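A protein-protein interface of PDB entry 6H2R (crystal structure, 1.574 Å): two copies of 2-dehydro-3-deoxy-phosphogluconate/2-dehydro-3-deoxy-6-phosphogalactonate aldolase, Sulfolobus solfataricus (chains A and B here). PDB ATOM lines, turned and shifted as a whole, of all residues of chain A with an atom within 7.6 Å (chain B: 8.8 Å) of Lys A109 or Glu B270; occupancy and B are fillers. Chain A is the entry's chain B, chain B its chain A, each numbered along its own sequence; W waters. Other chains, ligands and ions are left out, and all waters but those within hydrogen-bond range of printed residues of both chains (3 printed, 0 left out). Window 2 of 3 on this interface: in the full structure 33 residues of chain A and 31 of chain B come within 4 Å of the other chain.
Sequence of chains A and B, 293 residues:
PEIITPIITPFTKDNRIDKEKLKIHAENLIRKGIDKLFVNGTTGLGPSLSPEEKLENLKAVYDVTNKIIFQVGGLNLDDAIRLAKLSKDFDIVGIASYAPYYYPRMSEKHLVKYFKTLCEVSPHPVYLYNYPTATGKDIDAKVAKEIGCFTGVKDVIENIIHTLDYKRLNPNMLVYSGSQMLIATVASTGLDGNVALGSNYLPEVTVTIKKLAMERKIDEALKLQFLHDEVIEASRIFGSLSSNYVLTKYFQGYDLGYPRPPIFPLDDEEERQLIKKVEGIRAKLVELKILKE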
ATOM      1  N   MET A 106     -10.531  -9.729  15.861  1.00  0.00           N
ATOM      2  CA  MET A 106      -9.822 -10.519  14.868  1.00  0.00           C
ATOM      3  C   MET A 106      -8.334 -10.515  15.203  1.00  0.00           C
ATOM      4  O   MET A 106      -7.756  -9.485  15.568  1.00  0.00           O
ATOM      5  CB  MET A 106     -10.058  -9.981  13.450  1.00  0.00           C
ATOM      6  CG  MET A 106     -11.504 -10.101  12.992  1.00  0.00           C
ATOM      7  SD  MET A 106     -11.767  -9.563  11.277  1.00  0.00           S
ATOM      8  CE  MET A 106     -10.659 -10.669  10.397  1.00  0.00           C
ATOM      9  N   SER A 107      -7.705 -11.686  15.085  1.00  0.00           N
ATOM     10  CA  SER A 107      -6.293 -11.780  15.458  1.00  0.00           C
ATOM     11  C   SER A 107      -5.408 -11.043  14.461  1.00  0.00           C
ATOM     12  O   SER A 107      -5.733 -10.937  13.273  1.00  0.00           O
ATOM     13  CB  SER A 107      -5.863 -13.246  15.524  1.00  0.00           C
ATOM     14  OG  SER A 107      -5.798 -13.826  14.240  1.00  0.00           O
ATOM     15  N   GLU A 108      -4.269 -10.545  14.959  1.00  0.00           N
ATOM     16  CA  GLU A 108      -3.265  -9.968  14.075  1.00  0.00           C
ATOM     17  C   GLU A 108      -2.845 -10.971  13.012  1.00  0.00           C
ATOM     18  O   GLU A 108      -2.690 -10.615  11.837  1.00  0.00           O
ATOM     19  CB  GLU A 108      -2.049  -9.491  14.875  1.00  0.00           C
ATOM     20  CG  GLU A 108      -1.005  -8.767  14.031  1.00  0.00           C
ATOM     21  CD  GLU A 108       0.215  -8.344  14.820  1.00  0.00           C
ATOM     22  OE1 GLU A 108       1.316  -8.842  14.522  1.00  0.00           O
ATOM     23  OE2 GLU A 108       0.071  -7.513  15.746  1.00  0.00           O
ATOM     24  N   LYS A 109      -2.669 -12.242  13.394  1.00  0.00           N
ATOM     25  CA  LYS A 109      -2.284 -13.259  12.425  1.00  0.00           C
ATOM     26  C   LYS A 109      -3.246 -13.307  11.248  1.00  0.00           C
ATOM     27  O   LYS A 109      -2.826 -13.393  10.093  1.00  0.00           O
ATOM     28  CB  LYS A 109      -2.207 -14.622  13.115  1.00  0.00           C
ATOM     29  CG  LYS A 109      -2.173 -15.782  12.150  1.00  0.00           C
ATOM     30  CD  LYS A 109      -1.818 -17.083  12.865  1.00  0.00           C
ATOM     31  CE  LYS A 109      -2.848 -17.441  13.923  1.00  0.00           C
ATOM     32  NZ  LYS A 109      -4.095 -17.965  13.324  1.00  0.00           N
ATOM     33  N   HIS A 110      -4.556 -13.274  11.530  1.00  0.00           N
ATOM     34  CA  HIS A 110      -5.548 -13.365  10.468  1.00  0.00           C
ATOM     35  C   HIS A 110      -5.584 -12.075   9.645  1.00  0.00           C
ATOM     36  O   HIS A 110      -5.745 -12.122   8.418  1.00  0.00           O
ATOM     37  CB  HIS A 110      -6.928 -13.659  11.050  1.00  0.00           C
ATOM     38  CG  HIS A 110      -7.082 -15.079  11.511  1.00  0.00           C
ATOM     39  ND1 HIS A 110      -8.182 -15.516  12.220  1.00  0.00           N
ATOM     40  CD2 HIS A 110      -6.258 -16.150  11.379  1.00  0.00           C
ATOM     41  CE1 HIS A 110      -8.045 -16.813  12.475  1.00  0.00           C
ATOM     42  NE2 HIS A 110      -6.888 -17.225  11.976  1.00  0.00           N
ATOM     43  N   LEU A 111      -5.408 -10.930  10.306  1.00  0.00           N
ATOM     44  CA  LEU A 111      -5.356  -9.654   9.585  1.00  0.00           C
ATOM     45  C   LEU A 111      -4.158  -9.626   8.646  1.00  0.00           C
ATOM     46  O   LEU A 111      -4.278  -9.211   7.490  1.00  0.00           O
ATOM     47  CB  LEU A 111      -5.310  -8.480  10.554  1.00  0.00           C
ATOM     48  CG  LEU A 111      -6.562  -8.318  11.394  1.00  0.00           C
ATOM     49  CD1 LEU A 111      -6.389  -7.357  12.552  1.00  0.00           C
ATOM     50  CD2 LEU A 111      -7.753  -7.910  10.509  1.00  0.00           C
ATOM     51  N   VAL A 112      -2.987 -10.040   9.142  1.00  0.00           N
ATOM     52  CA  VAL A 112      -1.788 -10.104   8.307  1.00  0.00           C
ATOM     53  C   VAL A 112      -2.002 -11.033   7.125  1.00  0.00           C
ATOM     54  O   VAL A 112      -1.632 -10.720   5.985  1.00  0.00           O
ATOM     55  CB  VAL A 112      -0.578 -10.540   9.164  1.00  0.00           C
ATOM     56  CG1 VAL A 112       0.597 -10.890   8.258  1.00  0.00           C
ATOM     57  CG2 VAL A 112      -0.223  -9.469  10.166  1.00  0.00           C
ATOM     58  N   LYS A 113      -2.615 -12.192   7.364  1.00  0.00           N
ATOM     59  CA  LYS A 113      -2.789 -13.162   6.295  1.00  0.00           C
ATOM     60  C   LYS A 113      -3.703 -12.614   5.209  1.00  0.00           C
ATOM     61  O   LYS A 113      -3.499 -12.868   4.011  1.00  0.00           O
ATOM     62  CB  LYS A 113      -3.347 -14.474   6.873  1.00  0.00           C
ATOM     63  CG  LYS A 113      -3.490 -15.570   5.894  1.00  0.00           C
ATOM     64  CD  LYS A 113      -3.933 -16.849   6.599  1.00  0.00           C
ATOM     65  CE  LYS A 113      -3.876 -18.063   5.698  1.00  0.00           C
ATOM     66  NZ  LYS A 113      -2.466 -18.429   5.396  1.00  0.00           N
ATOM     67  N   TYR A 114      -4.755 -11.897   5.610  1.00  0.00           N
ATOM     68  CA  TYR A 114      -5.622 -11.251   4.633  1.00  0.00           C
ATOM     69  C   TYR A 114      -4.822 -10.358   3.690  1.00  0.00           C
ATOM     70  O   TYR A 114      -4.948 -10.475   2.468  1.00  0.00           O
ATOM     71  CB  TYR A 114      -6.712 -10.463   5.368  1.00  0.00           C
ATOM     72  CG  TYR A 114      -7.569  -9.597   4.477  1.00  0.00           C
ATOM     73  CD1 TYR A 114      -8.641 -10.116   3.767  1.00  0.00           C
ATOM     74  CD2 TYR A 114      -7.265  -8.269   4.288  1.00  0.00           C
ATOM     75  CE1 TYR A 114      -9.447  -9.305   2.935  1.00  0.00           C
ATOM     76  CE2 TYR A 114      -8.052  -7.441   3.451  1.00  0.00           C
ATOM     77  CZ  TYR A 114      -9.122  -7.968   2.774  1.00  0.00           C
ATOM     78  OH  TYR A 114      -9.896  -7.207   1.963  1.00  0.00           O
ATOM     79  N   PHE A 115      -4.003  -9.448   4.236  1.00  0.00           N
ATOM     80  CA  PHE A 115      -3.281  -8.515   3.374  1.00  0.00           C
ATOM     81  C   PHE A 115      -2.199  -9.221   2.564  1.00  0.00           C
ATOM     82  O   PHE A 115      -2.036  -8.931   1.372  1.00  0.00           O
ATOM     83  CB  PHE A 115      -2.703  -7.394   4.219  1.00  0.00           C
ATOM     84  CG  PHE A 115      -3.732  -6.391   4.666  1.00  0.00           C
ATOM     85  CD1 PHE A 115      -4.289  -5.510   3.746  1.00  0.00           C
ATOM     86  CD2 PHE A 115      -4.186  -6.348   5.973  1.00  0.00           C
ATOM     87  CE1 PHE A 115      -5.221  -4.582   4.134  1.00  0.00           C
ATOM     88  CE2 PHE A 115      -5.133  -5.447   6.349  1.00  0.00           C
ATOM     89  CZ  PHE A 115      -5.637  -4.544   5.444  1.00  0.00           C
ATOM     90  N   LYS A 116      -1.484 -10.185   3.173  1.00  0.00           N
ATOM     91  CA  LYS A 116      -0.430 -10.872   2.417  1.00  0.00           C
ATOM     92  C   LYS A 116      -1.022 -11.661   1.265  1.00  0.00           C
ATOM     93  O   LYS A 116      -0.400 -11.770   0.213  1.00  0.00           O
ATOM     94  CB  LYS A 116       0.388 -11.777   3.322  1.00  0.00           C
ATOM     95  CG  LYS A 116       1.300 -11.010   4.266  1.00  0.00           C
ATOM     96  CD  LYS A 116       2.166 -11.921   5.132  1.00  0.00           C
ATOM     97  CE  LYS A 116       3.520 -12.179   4.519  1.00  0.00           C
ATOM     98  NZ  LYS A 116       4.413 -12.835   5.535  1.00  0.00           N
ATOM     99  N   VAL A 143       2.412  -3.365  12.316  1.00  0.00           N
ATOM    100  CA  VAL A 143       1.750  -4.446  11.598  1.00  0.00           C
ATOM    101  C   VAL A 143       1.986  -4.302  10.098  1.00  0.00           C
ATOM    102  O   VAL A 143       2.211  -5.293   9.395  1.00  0.00           O
ATOM    103  CB  VAL A 143       0.250  -4.480  11.929  1.00  0.00           C
ATOM    104  CG1 VAL A 143      -0.450  -5.648  11.224  1.00  0.00           C
ATOM    105  CG2 VAL A 143       0.052  -4.584  13.443  1.00  0.00           C
ATOM    106  N   ALA B 234     -11.407 -20.484  26.039  1.00  0.00           N
ATOM    107  CA  ALA B 234     -10.490 -21.197  25.161  1.00  0.00           C
ATOM    108  C   ALA B 234     -10.738 -20.852  23.696  1.00  0.00           C
ATOM    109  O   ALA B 234      -9.790 -20.734  22.900  1.00  0.00           O
ATOM    110  CB  ALA B 234     -10.617 -22.701  25.400  1.00  0.00           C
ATOM    111  N   ILE B 237      -8.811 -17.857  22.225  1.00  0.00           N
ATOM    112  CA  ILE B 237      -7.364 -17.856  22.072  1.00  0.00           C
ATOM    113  C   ILE B 237      -6.979 -17.660  20.616  1.00  0.00           C
ATOM    114  O   ILE B 237      -6.099 -16.857  20.289  1.00  0.00           O
ATOM    115  CB  ILE B 237      -6.754 -19.151  22.649  1.00  0.00           C
ATOM    116  CG1 ILE B 237      -7.002 -19.164  24.151  1.00  0.00           C
ATOM    117  CG2 ILE B 237      -5.252 -19.249  22.341  1.00  0.00           C
ATOM    118  CD1 ILE B 237      -6.655 -20.482  24.778  1.00  0.00           C
ATOM    119  N   PHE B 238      -7.627 -18.400  19.704  1.00  0.00           N
ATOM    120  CA  PHE B 238      -7.255 -18.309  18.296  1.00  0.00           C
ATOM    121  C   PHE B 238      -8.326 -17.652  17.453  1.00  0.00           C
ATOM    122  O   PHE B 238      -8.170 -17.581  16.226  1.00  0.00           O
ATOM    123  CB  PHE B 238      -6.930 -19.690  17.719  1.00  0.00           C
ATOM    124  CG  PHE B 238      -5.811 -20.394  18.442  1.00  0.00           C
ATOM    125  CD1 PHE B 238      -4.526 -19.892  18.405  1.00  0.00           C
ATOM    126  CD2 PHE B 238      -6.058 -21.529  19.175  1.00  0.00           C
ATOM    127  CE1 PHE B 238      -3.503 -20.526  19.087  1.00  0.00           C
ATOM    128  CE2 PHE B 238      -5.033 -22.166  19.868  1.00  0.00           C
ATOM    129  CZ  PHE B 238      -3.766 -21.662  19.809  1.00  0.00           C
ATOM    130  N   GLY B 239      -9.397 -17.156  18.077  1.00  0.00           N
ATOM    131  CA  GLY B 239     -10.470 -16.494  17.349  1.00  0.00           C
ATOM    132  C   GLY B 239     -11.763 -17.278  17.481  1.00  0.00           C
ATOM    133  O   GLY B 239     -11.845 -18.400  16.981  1.00  0.00           O
ATOM    134  N   SER B 242     -13.775 -18.667  14.302  1.00  0.00           N
ATOM    135  CA  SER B 242     -13.091 -19.808  13.701  1.00  0.00           C
ATOM    136  C   SER B 242     -13.105 -21.019  14.627  1.00  0.00           C
ATOM    137  O   SER B 242     -13.328 -22.157  14.180  1.00  0.00           O
ATOM    138  CB  SER B 242     -11.651 -19.443  13.388  1.00  0.00           C
ATOM    139  OG  SER B 242     -11.552 -18.319  12.539  1.00  0.00           O
ATOM    140  N   SER B 243     -12.894 -20.792  15.922  1.00  0.00           N
ATOM    141  CA  SER B 243     -12.860 -21.898  16.887  1.00  0.00           C
ATOM    142  C   SER B 243     -14.198 -22.618  16.977  1.00  0.00           C
ATOM    143  O   SER B 243     -14.246 -23.834  17.260  1.00  0.00           O
ATOM    144  CB  SER B 243     -12.446 -21.388  18.260  1.00  0.00           C
ATOM    145  OG  SER B 243     -11.151 -20.883  18.227  1.00  0.00           O
ATOM    146  N   VAL B 246     -14.173 -25.907  15.057  1.00  0.00           N
ATOM    147  CA  VAL B 246     -13.420 -26.988  15.696  1.00  0.00           C
ATOM    148  C   VAL B 246     -14.187 -27.523  16.884  1.00  0.00           C
ATOM    149  O   VAL B 246     -14.270 -28.744  17.096  1.00  0.00           O
ATOM    150  CB  VAL B 246     -12.023 -26.482  16.101  1.00  0.00           C
ATOM    151  CG1 VAL B 246     -11.341 -27.468  17.029  1.00  0.00           C
ATOM    152  CG2 VAL B 246     -11.192 -26.214  14.877  1.00  0.00           C
ATOM    153  N   LEU B 247     -14.779 -26.623  17.675  1.00  0.00           N
ATOM    154  CA  LEU B 247     -15.465 -27.065  18.885  1.00  0.00           C
ATOM    155  C   LEU B 247     -16.736 -27.837  18.558  1.00  0.00           C
ATOM    156  O   LEU B 247     -17.105 -28.776  19.273  1.00  0.00           O
ATOM    157  CB  LEU B 247     -15.751 -25.851  19.769  1.00  0.00           C
ATOM    158  CG  LEU B 247     -14.527 -25.127  20.347  1.00  0.00           C
ATOM    159  CD1 LEU B 247     -14.929 -23.822  20.990  1.00  0.00           C
ATOM    160  CD2 LEU B 247     -13.792 -26.052  21.334  1.00  0.00           C
ATOM    161  N   PRO B 262     -11.833 -13.610   5.386  1.00  0.00           N
ATOM    162  CA  PRO B 262     -10.767 -13.549   6.404  1.00  0.00           C
ATOM    163  C   PRO B 262     -11.058 -14.065   7.806  1.00  0.00           C
ATOM    164  O   PRO B 262     -10.241 -13.839   8.713  1.00  0.00           O
ATOM    165  CB  PRO B 262     -10.457 -12.046   6.465  1.00  0.00           C
ATOM    166  CG  PRO B 262     -11.741 -11.421   6.160  1.00  0.00           C
ATOM    167  CD  PRO B 262     -12.361 -12.278   5.072  1.00  0.00           C
ATOM    168  N   PHE B 264     -10.373 -16.996   9.045  1.00  0.00           N
ATOM    169  CA  PHE B 264      -9.597 -18.122   8.564  1.00  0.00           C
ATOM    170  C   PHE B 264      -9.802 -19.336   9.460  1.00  0.00           C
ATOM    171  O   PHE B 264      -9.980 -19.192  10.683  1.00  0.00           O
ATOM    172  CB  PHE B 264      -8.102 -17.763   8.542  1.00  0.00           C
ATOM    173  CG  PHE B 264      -7.715 -16.838   7.419  1.00  0.00           C
ATOM    174  CD1 PHE B 264      -7.525 -17.332   6.139  1.00  0.00           C
ATOM    175  CD2 PHE B 264      -7.556 -15.480   7.649  1.00  0.00           C
ATOM    176  CE1 PHE B 264      -7.164 -16.467   5.103  1.00  0.00           C
ATOM    177  CE2 PHE B 264      -7.200 -14.628   6.599  1.00  0.00           C
ATOM    178  CZ  PHE B 264      -7.017 -15.134   5.362  1.00  0.00           C
ATOM    179  N   PRO B 265      -9.770 -20.532   8.886  1.00  0.00           N
ATOM    180  CA  PRO B 265      -9.793 -21.735   9.730  1.00  0.00           C
ATOM    181  C   PRO B 265      -8.580 -21.828  10.637  1.00  0.00           C
ATOM    182  O   PRO B 265      -7.475 -21.397  10.284  1.00  0.00           O
ATOM    183  CB  PRO B 265      -9.806 -22.885   8.722  1.00  0.00           C
ATOM    184  CG  PRO B 265      -9.182 -22.332   7.515  1.00  0.00           C
ATOM    185  CD  PRO B 265      -9.587 -20.849   7.467  1.00  0.00           C
ATOM    186  N   LEU B 266      -8.799 -22.434  11.796  1.00  0.00           N
ATOM    187  CA  LEU B 266      -7.704 -22.829  12.668  1.00  0.00           C
ATOM    188  C   LEU B 266      -6.788 -23.765  11.897  1.00  0.00           C
ATOM    189  O   LEU B 266      -7.264 -24.611  11.142  1.00  0.00           O
ATOM    190  CB  LEU B 266      -8.242 -23.516  13.924  1.00  0.00           C
ATOM    191  CG  LEU B 266      -8.377 -22.583  15.138  1.00  0.00           C
ATOM    192  CD1 LEU B 266      -9.329 -21.437  14.861  1.00  0.00           C
ATOM    193  CD2 LEU B 266      -8.783 -23.332  16.366  1.00  0.00           C
ATOM    194  N   ASP B 267      -5.480 -23.574  12.043  1.00  0.00           N
ATOM    195  CA  ASP B 267      -4.561 -24.524  11.406  1.00  0.00           C
ATOM    196  C   ASP B 267      -4.408 -25.748  12.304  1.00  0.00           C
ATOM    197  O   ASP B 267      -5.017 -25.849  13.360  1.00  0.00           O
ATOM    198  CB  ASP B 267      -3.240 -23.852  11.044  1.00  0.00           C
ATOM    199  CG  ASP B 267      -2.419 -23.431  12.210  1.00  0.00           C
ATOM    200  OD1 ASP B 267      -2.567 -23.979  13.323  1.00  0.00           O
ATOM    201  OD2 ASP B 267      -1.555 -22.509  12.026  1.00  0.00           O
ATOM    202  N   ASP B 268      -3.628 -26.732  11.848  1.00  0.00           N
ATOM    203  CA  ASP B 268      -3.596 -28.019  12.540  1.00  0.00           C
ATOM    204  C   ASP B 268      -3.134 -27.872  13.976  1.00  0.00           C
ATOM    205  O   ASP B 268      -3.693 -28.501  14.887  1.00  0.00           O
ATOM    206  CB  ASP B 268      -2.682 -28.991  11.775  1.00  0.00           C
ATOM    207  CG  ASP B 268      -3.226 -29.407  10.431  1.00  0.00           C
ATOM    208  OD1 ASP B 268      -4.442 -29.272  10.174  1.00  0.00           O
ATOM    209  OD2 ASP B 268      -2.426 -29.896   9.607  1.00  0.00           O
ATOM    210  N   GLU B 269      -2.096 -27.082  14.190  1.00  0.00           N
ATOM    211  CA  GLU B 269      -1.532 -26.895  15.512  1.00  0.00           C
ATOM    212  C   GLU B 269      -2.507 -26.155  16.413  1.00  0.00           C
ATOM    213  O   GLU B 269      -2.671 -26.520  17.588  1.00  0.00           O
ATOM    214  CB  GLU B 269      -0.203 -26.159  15.415  1.00  0.00           C
ATOM    215  CG  GLU B 269       0.424 -25.772  16.754  1.00  0.00           C
ATOM    216  CD  GLU B 269       0.903 -26.960  17.543  1.00  0.00           C
ATOM    217  OE1 GLU B 269       0.905 -28.081  16.989  1.00  0.00           O
ATOM    218  OE2 GLU B 269       1.229 -26.764  18.738  1.00  0.00           O
ATOM    219  N   GLU B 270      -3.181 -25.132  15.871  1.00  0.00           N
ATOM    220  CA  GLU B 270      -4.183 -24.421  16.657  1.00  0.00           C
ATOM    221  C   GLU B 270      -5.318 -25.339  17.057  1.00  0.00           C
ATOM    222  O   GLU B 270      -5.784 -25.289  18.203  1.00  0.00           O
ATOM    223  CB  GLU B 270      -4.697 -23.212  15.867  1.00  0.00           C
ATOM    224  CG  GLU B 270      -3.678 -22.127  15.698  1.00  0.00           C
ATOM    225  CD  GLU B 270      -4.109 -21.066  14.694  1.00  0.00           C
ATOM    226  OE1 GLU B 270      -4.873 -21.366  13.771  1.00  0.00           O
ATOM    227  OE2 GLU B 270      -3.663 -19.906  14.840  1.00  0.00           O
ATOM    228  N   GLU B 271      -5.778 -26.166  16.138  1.00  0.00           N
ATOM    229  CA  GLU B 271      -6.844 -27.118  16.453  1.00  0.00           C
ATOM    230  C   GLU B 271      -6.417 -28.061  17.571  1.00  0.00           C
ATOM    231  O   GLU B 271      -7.199 -28.359  18.471  1.00  0.00           O
ATOM    232  CB  GLU B 271      -7.238 -27.891  15.204  1.00  0.00           C
ATOM    233  CG  GLU B 271      -8.203 -29.025  15.447  1.00  0.00           C
ATOM    234  CD  GLU B 271      -8.929 -29.461  14.181  1.00  0.00           C
ATOM    235  OE1 GLU B 271      -8.541 -29.009  13.078  1.00  0.00           O
ATOM    236  OE2 GLU B 271      -9.914 -30.214  14.302  1.00  0.00           O
ATOM    237  N   ARG B 272      -5.186 -28.579  17.509  1.00  0.00           N
ATOM    238  CA  ARG B 272      -4.757 -29.499  18.558  1.00  0.00           C
ATOM    239  C   ARG B 272      -4.630 -28.794  19.904  1.00  0.00           C
ATOM    240  O   ARG B 272      -5.023 -29.361  20.941  1.00  0.00           O
ATOM    241  CB  ARG B 272      -3.440 -30.168  18.164  1.00  0.00           C
ATOM    242  CG  ARG B 272      -3.623 -31.267  17.150  1.00  0.00           C
ATOM    243  CD  ARG B 272      -2.328 -32.062  16.946  1.00  0.00           C
ATOM    244  NE  ARG B 272      -1.240 -31.217  16.483  1.00  0.00           N
ATOM    245  CZ  ARG B 272      -0.872 -31.084  15.211  1.00  0.00           C
ATOM    246  NH1 ARG B 272      -1.502 -31.722  14.244  1.00  0.00           N
ATOM    247  NH2 ARG B 272       0.151 -30.291  14.901  1.00  0.00           N
ATOM    248  N   GLN B 273      -4.122 -27.561  19.914  1.00  0.00           N
ATOM    249  CA  GLN B 273      -4.017 -26.803  21.156  1.00  0.00           C
ATOM    250  C   GLN B 273      -5.387 -26.510  21.744  1.00  0.00           C
ATOM    251  O   GLN B 273      -5.580 -26.619  22.943  1.00  0.00           O
ATOM    252  CB  GLN B 273      -3.270 -25.515  20.926  1.00  0.00           C
ATOM    253  CG  GLN B 273      -1.757 -25.690  20.695  1.00  0.00           C
ATOM    254  CD  GLN B 273      -0.991 -24.381  20.829  1.00  0.00           C
ATOM    255  OE1 GLN B 273      -1.338 -23.508  21.632  1.00  0.00           O
ATOM    256  NE2 GLN B 273       0.072 -24.246  20.050  1.00  0.00           N
ATOM    257  N   LEU B 274      -6.356 -26.136  20.898  1.00  0.00           N
ATOM    258  CA  LEU B 274      -7.690 -25.862  21.403  1.00  0.00           C
ATOM    259  C   LEU B 274      -8.309 -27.111  22.011  1.00  0.00           C
ATOM    260  O   LEU B 274      -8.924 -27.048  23.079  1.00  0.00           O
ATOM    261  CB  LEU B 274      -8.558 -25.292  20.278  1.00  0.00           C
ATOM    262  CG  LEU B 274     -10.034 -25.033  20.611  1.00  0.00           C
ATOM    263  CD1 LEU B 274     -10.185 -24.127  21.842  1.00  0.00           C
ATOM    264  CD2 LEU B 274     -10.710 -24.420  19.397  1.00  0.00           C
ATOM    265  N   ILE B 275      -8.185 -28.249  21.332  1.00  0.00           N
ATOM    266  CA  ILE B 275      -8.722 -29.500  21.878  1.00  0.00           C
ATOM    267  C   ILE B 275      -8.066 -29.834  23.223  1.00  0.00           C
ATOM    268  O   ILE B 275      -8.750 -30.236  24.160  1.00  0.00           O
ATOM    269  CB  ILE B 275      -8.569 -30.636  20.850  1.00  0.00           C
ATOM    270  CG1 ILE B 275      -9.596 -30.430  19.735  1.00  0.00           C
ATOM    271  CG2 ILE B 275      -8.749 -31.996  21.517  1.00  0.00           C
ATOM    272  CD1 ILE B 275      -9.334 -31.258  18.494  1.00  0.00           C
ATOM    273  N   LYS B 276      -6.750 -29.663  23.335  1.00  0.00           N
ATOM    274  CA  LYS B 276      -6.080 -29.895  24.612  1.00  0.00           C
ATOM    275  C   LYS B 276      -6.689 -29.038  25.710  1.00  0.00           C
ATOM    276  O   LYS B 276      -6.839 -29.488  26.849  1.00  0.00           O
ATOM    277  CB  LYS B 276      -4.585 -29.613  24.479  1.00  0.00           C
ATOM    278  CG  LYS B 276      -3.782 -29.786  25.771  1.00  0.00           C
ATOM    279  CD  LYS B 276      -2.327 -29.384  25.569  1.00  0.00           C
ATOM    280  CE  LYS B 276      -1.486 -29.587  26.828  1.00  0.00           C
ATOM    281  NZ  LYS B 276      -1.777 -28.580  27.888  1.00  0.00           N
ATOM    282  N   LYS B 277      -7.072 -27.798  25.382  1.00  0.00           N
ATOM    283  CA  LYS B 277      -7.634 -26.914  26.394  1.00  0.00           C
ATOM    284  C   LYS B 277      -9.014 -27.317  26.855  1.00  0.00           C
ATOM    285  O   LYS B 277      -9.426 -26.930  27.952  1.00  0.00           O
ATOM    286  CB  LYS B 277      -7.655 -25.467  25.873  1.00  0.00           C
ATOM    287  CG  LYS B 277      -6.263 -24.931  25.628  1.00  0.00           C
ATOM    288  CD  LYS B 277      -6.216 -23.443  25.406  1.00  0.00           C
ATOM    289  CE  LYS B 277      -4.810 -22.907  25.708  1.00  0.00           C
ATOM    290  NZ  LYS B 277      -4.550 -22.838  27.180  1.00  0.00           N
HETATM  291  O   HOH W   1      -1.331 -20.062  13.001  1.00  0.00           O
HETATM  292  O   HOH W   2      -5.600 -16.411  15.213  1.00  0.00           O
HETATM  293  O   HOH W   3      -5.731 -19.721  11.724  1.00  0.00           O
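Water W1 lies within hydrogen-bond range of the side-chain carboxylate (OD2) of Asp B267 (2.6 Å), the side-chain carboxylate (OE2) of Glu B270 (3.0 Å) and the side-chain amino group (NZ) of Lys A109 (3.5 Å). Water W3 lies within hydrogen-bond range of OE1 of Glu B270, NE2 of His A110, O of Pro B265 and NZ of Lys A109. Water W2 lies within hydrogen-bond range of OG of Ser A107 (2.8 Å), NZ of Lys A109 (2.9 Å) and O of Phe B238 (3.0 Å).
NZ of Lys A109 is in salt-bridge range of OE2 of Glu B270 (2.5 Å).
Printed residues of chain B within 4 Å of Met A106: Pro B262 (3.6 Å). Lys A109 touches one residue of chain B. Of the printed residues of chain B, Tyr A114 touches Pro B262 and Phe B264. Of the printed residues of chain A, Phe B238 touches His A110. Printed residues of chain A within 4 Å of Phe B264: His A110 (3.4 Å), Lys A113 (3.6 Å) and Tyr A114 (3.8 Å). The nearest printed residue of chain A that does not touch Ser B242 is Ser A107 (7.5 Å).
Printed residues of chain B that touch a printed residue of chain A: Phe B238, Ser B242, Pro B262, Phe B264 and Glu B270. Hydrophobic or aromatic side chains of chain B that line the printed part of chain A: Pro B262 and Phe B264. Along chain B the printed residues that touch a printed residue of chain A span positions 238 to 270. Of the 12 printed residues of chain A, 5 touch a printed residue of chain B. Hydrophobic or aromatic side chains of chain A that line the printed part of chain B: Met A106, His A110 and Tyr A114. Among the printed residues, 8 pairs touch across the chains. Among the printed residues, Asp or Glu carboxylates within 4 Å of a Lys or Arg side-chain nitrogen of the other chain: Lys A109 with Glu B270 (2.5 Å).
Met A106 touches Pro B262 (CE to O, 3.6 Å). CE1 of His A110 touches O of Phe B238 (3.8 Å). His A110 touches Ser B242 (CE1 to OG, 3.8 Å). O of His A110 touches CE2 of Phe B264, 3.4 Å away. Lys A113 touches Phe B264 (CD to CE1, 3.6 Å). CD1 of Tyr A114 touches CB of Pro B262, 3.8 Å away. Tyr A114 touches Phe B264.
The side-chain hydroxyl (OG) of Ser B242 sits at hydrogen-bond distance from the backbone carbonyl oxygen (O) of Phe B264, at 2.6 Å. OD1 of Asp B267 lies within hydrogen-bond range of N of Glu B270 (2.9 Å). The side-chain hydroxyl (OG) of Ser A107 lies within hydrogen-bond range of the backbone NH (N) of His A110 (3.0 Å). The side-chain amino group of Lys A109 lies within hydrogen-bond range of a ring nitrogen (NE2) of His A110 (3.2 Å).
No position is printed for both chains.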
